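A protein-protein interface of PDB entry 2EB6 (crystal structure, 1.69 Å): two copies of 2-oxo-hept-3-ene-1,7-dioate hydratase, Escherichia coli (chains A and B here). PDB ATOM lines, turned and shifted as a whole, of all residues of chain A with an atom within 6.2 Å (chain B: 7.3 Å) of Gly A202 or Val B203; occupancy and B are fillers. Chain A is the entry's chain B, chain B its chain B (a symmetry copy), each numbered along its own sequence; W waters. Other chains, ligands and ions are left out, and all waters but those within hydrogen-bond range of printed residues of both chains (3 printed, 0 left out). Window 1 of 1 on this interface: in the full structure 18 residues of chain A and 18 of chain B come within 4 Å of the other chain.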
ATOM      1  N   ILE A 188     -23.647  -0.066 -20.986  1.00  0.00           N
ATOM      2  CA  ILE A 188     -23.813   1.117 -20.141  1.00  0.00           C
ATOM      3  C   ILE A 188     -22.561   1.974 -20.302  1.00  0.00           C
ATOM      4  O   ILE A 188     -21.440   1.466 -20.253  1.00  0.00           O
ATOM      5  CB  ILE A 188     -24.056   0.731 -18.674  1.00  0.00           C
ATOM      6  CG1 ILE A 188     -25.440   0.090 -18.539  1.00  0.00           C
ATOM      7  CG2 ILE A 188     -23.973   1.960 -17.753  1.00  0.00           C
ATOM      8  CD1 ILE A 188     -25.685  -0.594 -17.215  1.00  0.00           C
ATOM      9  N   SER A 189     -22.754   3.268 -20.543  1.00  0.00           N
ATOM     10  CA  SER A 189     -21.623   4.157 -20.779  1.00  0.00           C
ATOM     11  C   SER A 189     -21.757   5.429 -19.958  1.00  0.00           C
ATOM     12  O   SER A 189     -22.843   5.749 -19.469  1.00  0.00           O
ATOM     13  CB  SER A 189     -21.485   4.476 -22.264  1.00  0.00           C
ATOM     14  OG  SER A 189     -22.602   5.199 -22.727  1.00  0.00           O
ATOM     15  N   ALA A 190     -20.647   6.142 -19.800  1.00  0.00           N
ATOM     16  CA  ALA A 190     -20.608   7.279 -18.889  1.00  0.00           C
ATOM     17  C   ALA A 190     -19.652   8.368 -19.337  1.00  0.00           C
ATOM     18  O   ALA A 190     -18.639   8.092 -19.993  1.00  0.00           O
ATOM     19  CB  ALA A 190     -20.261   6.824 -17.487  1.00  0.00           C
ATOM     20  N   LEU A 191     -20.009   9.605 -18.979  1.00  0.00           N
ATOM     21  CA  LEU A 191     -19.173  10.788 -19.159  1.00  0.00           C
ATOM     22  C   LEU A 191     -18.849  11.340 -17.771  1.00  0.00           C
ATOM     23  O   LEU A 191     -19.772  11.650 -17.011  1.00  0.00           O
ATOM     24  CB  LEU A 191     -19.947  11.854 -19.944  1.00  0.00           C
ATOM     25  CG  LEU A 191     -20.668  11.428 -21.228  1.00  0.00           C
ATOM     26  CD1 LEU A 191     -21.557  12.567 -21.745  1.00  0.00           C
ATOM     27  CD2 LEU A 191     -19.690  10.986 -22.311  1.00  0.00           C
ATOM     28  N   GLU A 200     -12.977  12.140 -18.459  1.00  0.00           N
ATOM     29  CA  GLU A 200     -12.916  10.754 -18.943  1.00  0.00           C
ATOM     30  C   GLU A 200     -14.278  10.300 -19.453  1.00  0.00           C
ATOM     31  O   GLU A 200     -15.312  10.787 -19.002  1.00  0.00           O
ATOM     32  CB  GLU A 200     -12.467   9.779 -17.833  1.00  0.00           C
ATOM     33  CG  GLU A 200     -11.063  10.001 -17.242  1.00  0.00           C
ATOM     34  CD  GLU A 200      -9.910   9.709 -18.204  1.00  0.00           C
ATOM     35  OE1 GLU A 200     -10.100   9.008 -19.229  1.00  0.00           O
ATOM     36  OE2 GLU A 200      -8.786  10.185 -17.918  1.00  0.00           O
ATOM     37  N   THR A 201     -14.270   9.360 -20.394  1.00  0.00           N
ATOM     38  CA  THR A 201     -15.491   8.651 -20.779  1.00  0.00           C
ATOM     39  C   THR A 201     -15.173   7.161 -20.799  1.00  0.00           C
ATOM     40  O   THR A 201     -14.005   6.773 -20.879  1.00  0.00           O
ATOM     41  CB  THR A 201     -16.026   9.087 -22.165  1.00  0.00           C
ATOM     42  OG1 THR A 201     -15.125   8.656 -23.197  1.00  0.00           O
ATOM     43  CG2 THR A 201     -16.205  10.605 -22.235  1.00  0.00           C
ATOM     44  N   GLY A 202     -16.207   6.330 -20.738  1.00  0.00           N
ATOM     45  CA  GLY A 202     -15.986   4.888 -20.735  1.00  0.00           C
ATOM     46  C   GLY A 202     -17.245   4.079 -20.912  1.00  0.00           C
ATOM     47  O   GLY A 202     -18.360   4.598 -20.805  1.00  0.00           O
ATOM     48  N   VAL A 203     -17.049   2.796 -21.195  1.00  0.00           N
ATOM     49  CA  VAL A 203     -18.154   1.859 -21.406  1.00  0.00           C
ATOM     50  C   VAL A 203     -17.936   0.650 -20.497  1.00  0.00           C
ATOM     51  O   VAL A 203     -16.800   0.213 -20.319  1.00  0.00           O
ATOM     52  CB  VAL A 203     -18.248   1.431 -22.899  1.00  0.00           C
ATOM     53  CG1 VAL A 203     -19.464   0.530 -23.135  1.00  0.00           C
ATOM     54  CG2 VAL A 203     -18.334   2.666 -23.819  1.00  0.00           C
ATOM     55  N   ALA A 204     -19.024   0.112 -19.943  1.00  0.00           N
ATOM     56  CA  ALA A 204     -18.945  -0.909 -18.886  1.00  0.00           C
ATOM     57  C   ALA A 204     -18.214  -2.188 -19.282  1.00  0.00           C
ATOM     58  O   ALA A 204     -17.612  -2.840 -18.429  1.00  0.00           O
ATOM     59  CB  ALA A 204     -20.331  -1.240 -18.363  1.00  0.00           C
ATOM     60  N   PHE A 240     -14.823   1.885 -15.237  1.00  0.00           N
ATOM     61  CA  PHE A 240     -14.597   1.892 -16.675  1.00  0.00           C
ATOM     62  C   PHE A 240     -13.813   3.097 -17.193  1.00  0.00           C
ATOM     63  O   PHE A 240     -13.617   3.262 -18.396  1.00  0.00           O
ATOM     64  CB  PHE A 240     -15.798   1.463 -17.543  1.00  0.00           C
ATOM     65  CG  PHE A 240     -17.175   1.858 -17.021  1.00  0.00           C
ATOM     66  CD1 PHE A 240     -17.883   2.891 -17.625  1.00  0.00           C
ATOM     67  CD2 PHE A 240     -17.803   1.117 -16.022  1.00  0.00           C
ATOM     68  CE1 PHE A 240     -19.155   3.220 -17.209  1.00  0.00           C
ATOM     69  CE2 PHE A 240     -19.093   1.424 -15.604  1.00  0.00           C
ATOM     70  CZ  PHE A 240     -19.771   2.495 -16.200  1.00  0.00           C
ATOM     71  N   THR A 241     -13.309   3.891 -16.249  1.00  0.00           N
ATOM     72  CA  THR A 241     -12.446   5.037 -16.554  1.00  0.00           C
ATOM     73  C   THR A 241     -11.201   5.045 -15.663  1.00  0.00           C
ATOM     74  O   THR A 241     -11.212   4.507 -14.548  1.00  0.00           O
ATOM     75  CB  THR A 241     -13.181   6.369 -16.302  1.00  0.00           C
ATOM     76  OG1 THR A 241     -13.615   6.412 -14.931  1.00  0.00           O
ATOM     77  CG2 THR A 241     -14.398   6.513 -17.230  1.00  0.00           C
ATOM     78  N   LEU B 185     -25.538  11.934 -31.775  1.00  0.00           N
ATOM     79  CA  LEU B 185     -24.130  11.602 -32.001  1.00  0.00           C
ATOM     80  C   LEU B 185     -23.296  11.605 -30.730  1.00  0.00           C
ATOM     81  O   LEU B 185     -22.273  10.908 -30.655  1.00  0.00           O
ATOM     82  CB  LEU B 185     -23.499  12.540 -33.031  1.00  0.00           C
ATOM     83  CG  LEU B 185     -24.185  12.653 -34.390  1.00  0.00           C
ATOM     84  CD1 LEU B 185     -23.382  13.612 -35.258  1.00  0.00           C
ATOM     85  CD2 LEU B 185     -24.333  11.290 -35.074  1.00  0.00           C
ATOM     86  N   ARG B 186     -23.740  12.374 -29.731  1.00  0.00           N
ATOM     87  CA  ARG B 186     -23.007  12.517 -28.471  1.00  0.00           C
ATOM     88  C   ARG B 186     -22.827  11.196 -27.741  1.00  0.00           C
ATOM     89  O   ARG B 186     -21.854  11.023 -27.016  1.00  0.00           O
ATOM     90  CB  ARG B 186     -23.711  13.506 -27.544  1.00  0.00           C
ATOM     91  CG  ARG B 186     -23.742  14.919 -28.080  1.00  0.00           C
ATOM     92  CD  ARG B 186     -24.749  15.789 -27.332  1.00  0.00           C
ATOM     93  NE  ARG B 186     -24.488  15.858 -25.898  1.00  0.00           N
ATOM     94  CZ  ARG B 186     -25.163  15.187 -24.969  1.00  0.00           C
ATOM     95  NH1 ARG B 186     -26.173  14.380 -25.302  1.00  0.00           N
ATOM     96  NH2 ARG B 186     -24.833  15.331 -23.695  1.00  0.00           N
ATOM     97  N   TRP B 187     -23.767  10.273 -27.933  1.00  0.00           N
ATOM     98  CA  TRP B 187     -23.769   9.036 -27.156  1.00  0.00           C
ATOM     99  C   TRP B 187     -23.288   7.804 -27.911  1.00  0.00           C
ATOM    100  O   TRP B 187     -23.364   6.685 -27.396  1.00  0.00           O
ATOM    101  CB  TRP B 187     -25.145   8.801 -26.525  1.00  0.00           C
ATOM    102  CG  TRP B 187     -25.327   9.574 -25.272  1.00  0.00           C
ATOM    103  CD1 TRP B 187     -26.080  10.703 -25.104  1.00  0.00           C
ATOM    104  CD2 TRP B 187     -24.708   9.309 -24.010  1.00  0.00           C
ATOM    105  NE1 TRP B 187     -25.985  11.146 -23.801  1.00  0.00           N
ATOM    106  CE2 TRP B 187     -25.150  10.306 -23.109  1.00  0.00           C
ATOM    107  CE3 TRP B 187     -23.837   8.315 -23.546  1.00  0.00           C
ATOM    108  CZ2 TRP B 187     -24.740  10.342 -21.768  1.00  0.00           C
ATOM    109  CZ3 TRP B 187     -23.433   8.351 -22.210  1.00  0.00           C
ATOM    110  CH2 TRP B 187     -23.884   9.358 -21.341  1.00  0.00           C
ATOM    111  N   ILE B 188     -22.776   8.004 -29.122  1.00  0.00           N
ATOM    112  CA  ILE B 188     -22.095   6.913 -29.819  1.00  0.00           C
ATOM    113  C   ILE B 188     -20.904   6.494 -28.962  1.00  0.00           C
ATOM    114  O   ILE B 188     -20.150   7.338 -28.477  1.00  0.00           O
ATOM    115  CB  ILE B 188     -21.662   7.333 -31.232  1.00  0.00           C
ATOM    116  CG1 ILE B 188     -22.902   7.504 -32.115  1.00  0.00           C
ATOM    117  CG2 ILE B 188     -20.729   6.286 -31.865  1.00  0.00           C
ATOM    118  CD1 ILE B 188     -22.639   8.191 -33.434  1.00  0.00           C
ATOM    119  N   SER B 189     -20.764   5.191 -28.737  1.00  0.00           N
ATOM    120  CA  SER B 189     -19.698   4.695 -27.875  1.00  0.00           C
ATOM    121  C   SER B 189     -18.975   3.529 -28.529  1.00  0.00           C
ATOM    122  O   SER B 189     -19.487   2.922 -29.473  1.00  0.00           O
ATOM    123  CB  SER B 189     -20.245   4.303 -26.507  1.00  0.00           C
ATOM    124  OG  SER B 189     -21.139   3.219 -26.617  1.00  0.00           O
ATOM    125  N   ALA B 190     -17.781   3.229 -28.030  1.00  0.00           N
ATOM    126  CA  ALA B 190     -16.917   2.253 -28.684  1.00  0.00           C
ATOM    127  C   ALA B 190     -16.035   1.494 -27.712  1.00  0.00           C
ATOM    128  O   ALA B 190     -15.652   2.020 -26.659  1.00  0.00           O
ATOM    129  CB  ALA B 190     -16.070   2.923 -29.745  1.00  0.00           C
ATOM    130  N   LEU B 191     -15.738   0.247 -28.087  1.00  0.00           N
ATOM    131  CA  LEU B 191     -14.783  -0.616 -27.397  1.00  0.00           C
ATOM    132  C   LEU B 191     -13.637  -0.904 -28.366  1.00  0.00           C
ATOM    133  O   LEU B 191     -13.883  -1.424 -29.459  1.00  0.00           O
ATOM    134  CB  LEU B 191     -15.458  -1.941 -27.025  1.00  0.00           C
ATOM    135  CG  LEU B 191     -16.826  -1.890 -26.336  1.00  0.00           C
ATOM    136  CD1 LEU B 191     -17.432  -3.297 -26.245  1.00  0.00           C
ATOM    137  CD2 LEU B 191     -16.744  -1.257 -24.950  1.00  0.00           C
ATOM    138  N   GLU B 200      -9.054   0.169 -24.699  1.00  0.00           N
ATOM    139  CA  GLU B 200      -9.699   1.451 -24.382  1.00  0.00           C
ATOM    140  C   GLU B 200     -11.191   1.393 -24.686  1.00  0.00           C
ATOM    141  O   GLU B 200     -11.627   0.643 -25.555  1.00  0.00           O
ATOM    142  CB  GLU B 200      -9.087   2.616 -25.190  1.00  0.00           C
ATOM    143  CG  GLU B 200      -7.595   2.913 -24.956  1.00  0.00           C
ATOM    144  CD  GLU B 200      -7.263   3.471 -23.571  1.00  0.00           C
ATOM    145  OE1 GLU B 200      -8.165   3.976 -22.857  1.00  0.00           O
ATOM    146  OE2 GLU B 200      -6.068   3.411 -23.196  1.00  0.00           O
ATOM    147  N   THR B 201     -11.969   2.196 -23.964  1.00  0.00           N
ATOM    148  CA  THR B 201     -13.367   2.435 -24.325  1.00  0.00           C
ATOM    149  C   THR B 201     -13.603   3.939 -24.282  1.00  0.00           C
ATOM    150  O   THR B 201     -12.839   4.674 -23.651  1.00  0.00           O
ATOM    151  CB  THR B 201     -14.362   1.725 -23.375  1.00  0.00           C
ATOM    152  OG1 THR B 201     -14.311   2.326 -22.072  1.00  0.00           O
ATOM    153  CG2 THR B 201     -14.052   0.230 -23.267  1.00  0.00           C
ATOM    154  N   GLY B 202     -14.664   4.395 -24.939  1.00  0.00           N
ATOM    155  CA  GLY B 202     -14.950   5.826 -24.961  1.00  0.00           C
ATOM    156  C   GLY B 202     -16.304   6.167 -25.528  1.00  0.00           C
ATOM    157  O   GLY B 202     -16.970   5.328 -26.142  1.00  0.00           O
ATOM    158  N   VAL B 203     -16.706   7.413 -25.304  1.00  0.00           N
ATOM    159  CA  VAL B 203     -17.995   7.920 -25.775  1.00  0.00           C
ATOM    160  C   VAL B 203     -17.746   9.213 -26.551  1.00  0.00           C
ATOM    161  O   VAL B 203     -16.891  10.007 -26.161  1.00  0.00           O
ATOM    162  CB  VAL B 203     -18.972   8.156 -24.587  1.00  0.00           C
ATOM    163  CG1 VAL B 203     -20.352   8.592 -25.090  1.00  0.00           C
ATOM    164  CG2 VAL B 203     -19.114   6.881 -23.731  1.00  0.00           C
ATOM    165  N   ALA B 204     -18.502   9.421 -27.630  1.00  0.00           N
ATOM    166  CA  ALA B 204     -18.228  10.505 -28.586  1.00  0.00           C
ATOM    167  C   ALA B 204     -18.260  11.909 -27.991  1.00  0.00           C
ATOM    168  O   ALA B 204     -17.553  12.795 -28.472  1.00  0.00           O
ATOM    169  CB  ALA B 204     -19.170  10.418 -29.772  1.00  0.00           C
ATOM    170  N   ALA B 205     -19.072  12.116 -26.955  1.00  0.00           N
ATOM    171  CA  ALA B 205     -19.154  13.441 -26.308  1.00  0.00           C
ATOM    172  C   ALA B 205     -17.809  13.869 -25.729  1.00  0.00           C
ATOM    173  O   ALA B 205     -17.572  15.057 -25.516  1.00  0.00           O
ATOM    174  CB  ALA B 205     -20.238  13.458 -25.223  1.00  0.00           C
ATOM    175  N   GLY B 206     -16.925  12.898 -25.490  1.00  0.00           N
ATOM    176  CA  GLY B 206     -15.556  13.170 -25.048  1.00  0.00           C
ATOM    177  C   GLY B 206     -14.747  13.989 -26.040  1.00  0.00           C
ATOM    178  O   GLY B 206     -13.673  14.507 -25.700  1.00  0.00           O
ATOM    179  N   VAL B 207     -15.261  14.094 -27.265  1.00  0.00           N
ATOM    180  CA  VAL B 207     -14.656  14.920 -28.304  1.00  0.00           C
ATOM    181  C   VAL B 207     -15.347  16.290 -28.295  1.00  0.00           C
ATOM    182  O   VAL B 207     -16.400  16.469 -28.917  1.00  0.00           O
ATOM    183  CB  VAL B 207     -14.785  14.268 -29.703  1.00  0.00           C
ATOM    184  CG1 VAL B 207     -14.154  15.154 -30.779  1.00  0.00           C
ATOM    185  CG2 VAL B 207     -14.142  12.866 -29.729  1.00  0.00           C
ATOM    186  N   PRO B 211     -19.101  15.604 -31.044  1.00  0.00           N
ATOM    187  CA  PRO B 211     -18.106  15.231 -32.054  1.00  0.00           C
ATOM    188  C   PRO B 211     -18.136  16.068 -33.335  1.00  0.00           C
ATOM    189  O   PRO B 211     -17.202  15.978 -34.136  1.00  0.00           O
ATOM    190  CB  PRO B 211     -18.423  13.754 -32.341  1.00  0.00           C
ATOM    191  CG  PRO B 211     -19.857  13.575 -31.919  1.00  0.00           C
ATOM    192  CD  PRO B 211     -20.030  14.495 -30.746  1.00  0.00           C
ATOM    193  N   SER B 239     -10.526  11.878 -31.435  1.00  0.00           N
ATOM    194  CA  SER B 239     -10.567  10.537 -30.866  1.00  0.00           C
ATOM    195  C   SER B 239     -11.312  10.517 -29.543  1.00  0.00           C
ATOM    196  O   SER B 239     -11.104  11.390 -28.688  1.00  0.00           O
ATOM    197  CB  SER B 239      -9.151  10.007 -30.658  1.00  0.00           C
ATOM    198  OG  SER B 239      -9.171   8.657 -30.209  1.00  0.00           O
ATOM    199  N   PHE B 240     -12.177   9.534 -29.338  1.00  0.00           N
ATOM    200  CA  PHE B 240     -12.730   9.468 -27.993  1.00  0.00           C
ATOM    201  C   PHE B 240     -11.984   8.538 -27.038  1.00  0.00           C
ATOM    202  O   PHE B 240     -12.390   8.335 -25.896  1.00  0.00           O
ATOM    203  CB  PHE B 240     -14.270   9.407 -27.906  1.00  0.00           C
ATOM    204  CG  PHE B 240     -14.972   8.639 -29.020  1.00  0.00           C
ATOM    205  CD1 PHE B 240     -15.512   7.382 -28.771  1.00  0.00           C
ATOM    206  CD2 PHE B 240     -15.200   9.227 -30.262  1.00  0.00           C
ATOM    207  CE1 PHE B 240     -16.207   6.700 -29.747  1.00  0.00           C
ATOM    208  CE2 PHE B 240     -15.914   8.560 -31.251  1.00  0.00           C
ATOM    209  CZ  PHE B 240     -16.415   7.278 -30.991  1.00  0.00           C
ATOM    210  N   THR B 241     -10.843   8.038 -27.515  1.00  0.00           N
ATOM    211  CA  THR B 241      -9.942   7.208 -26.707  1.00  0.00           C
ATOM    212  C   THR B 241      -8.493   7.683 -26.830  1.00  0.00           C
ATOM    213  O   THR B 241      -8.104   8.289 -27.838  1.00  0.00           O
ATOM    214  CB  THR B 241      -9.971   5.740 -27.176  1.00  0.00           C
ATOM    215  OG1 THR B 241      -9.600   5.685 -28.565  1.00  0.00           O
ATOM    216  CG2 THR B 241     -11.368   5.127 -26.993  1.00  0.00           C
HETATM  217  O   HOH W   1     -24.207   5.165 -25.225  1.00  0.00           O
HETATM  218  O   HOH W   2     -13.132   1.100 -20.057  1.00  0.00           O
HETATM  219  O   HOH W   3     -13.549  10.376 -24.427  1.00  0.00           O
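N of Ala A190 is in hydrogen-bond range of O of Gly A202 (2.9 Å).
O of Arg B186 sits at hydrogen-bond distance from N of Ala B205, 3.0 Å away.
O of Gly B202 is in hydrogen-bond range of N of Ala B190, 2.9 Å away.
Water W3 lies within hydrogen-bond range of the side-chain hydroxyl (OG1) of Thr A201 (2.6 Å) and the backbone carbonyl oxygen (O) of Phe B240 (2.8 Å).
Water W2 bridges OG1 of Thr B201 (2.6 Å) and O of Phe A240 (2.8 Å).
Water W1 lies within hydrogen-bond range of the backbone carbonyl oxygen of Trp B187 (2.8 Å) and the side-chain hydroxyl of Ser A189 (3.0 Å).
The backbone NH (N) of Val B203 is in hydrogen-bond range of the side-chain hydroxyl (OG1) of Thr A201, 2.9 Å away.
N of Val A203 lies within hydrogen-bond range of OG1 of Thr B201, at 2.9 Å.
Printed residues of chain A that touch a printed residue of chain B: Ser A189, Ala A190, Leu A191, Thr A201, Gly A202, Val A203 and Phe A240.
Hydrophobic or aromatic side chains of chain A that line the printed part of chain B: Leu A191 and Val A203.
Printed residues of chain B that touch a printed residue of chain A: Trp B187, Ser B189, Ala B190, Leu B191, Thr B201, Gly B202, Val B203, Ala B205, Gly B206 and Phe B240.
Among the printed residues, 19 pairs touch across the chains.
Ser A189 touches Val B203 (CB to CG2, 3.7 Å).
CG2 of Val B203 touches O of Ala A190 (3.96 Å).
Leu A191 touches Val B203.
Ala B205 touches Leu A191 (CB to CD1, 3.8 Å).
Thr A201 touches Gly B202.
OG1 of Thr A201 touches O of Phe B240, at 3.9 Å.
CA of Gly A202 touches OG1 of Thr B201, at 3.3 Å.
CB of Ser B189 touches CG2 of Val A203, at 3.7 Å.
Ala B190 touches Val A203 (O to CG2, 3.96 Å).
CD2 of Leu B191 touches CB of Val A203, at 3.7 Å.
Leu A191 touches Val B203, and with the chains exchanged Val A203 touches Leu B191.
Thr A201 touches its own counterpart, Thr B201.
Thr A201 touches Val B203, and with the chains exchanged Val A203 touches Thr B201.
Gly A202 touches Val B203, and with the chains exchanged Val A203 touches Gly B202.
Of the 19 pairs that touch across the chains among the printed residues, 15 have their exchanged pair printed and touching as well.
Printed residues of chain B within 4 Å of Thr A201: Thr B201 (3.7 Å), Gly B202 (3.3 Å), Val B203 (2.9 Å), Gly B206 (3.9 Å) and Phe B240 (3.9 Å).
Of chain B, only Thr B201 and Val B203 come within 4 Å of Gly A202.
Of the printed residues of chain B, Phe A240 touches Thr B201.
Printed residues of chain A within 4 Å of Leu B191: Val A203.
Of the printed residues of chain A, Val B203 touches Ser A189 (3.7 Å), Ala A190 (3.96 Å), Leu A191 (3.7 Å), Thr A201 (2.9 Å) and Gly A202 (3.8 Å).
Of the printed residues of chain A, Phe B240 touches Thr A201.
The nearest residue of chain B that does not touch Gly A202 is Gly B202 (4.4 Å).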
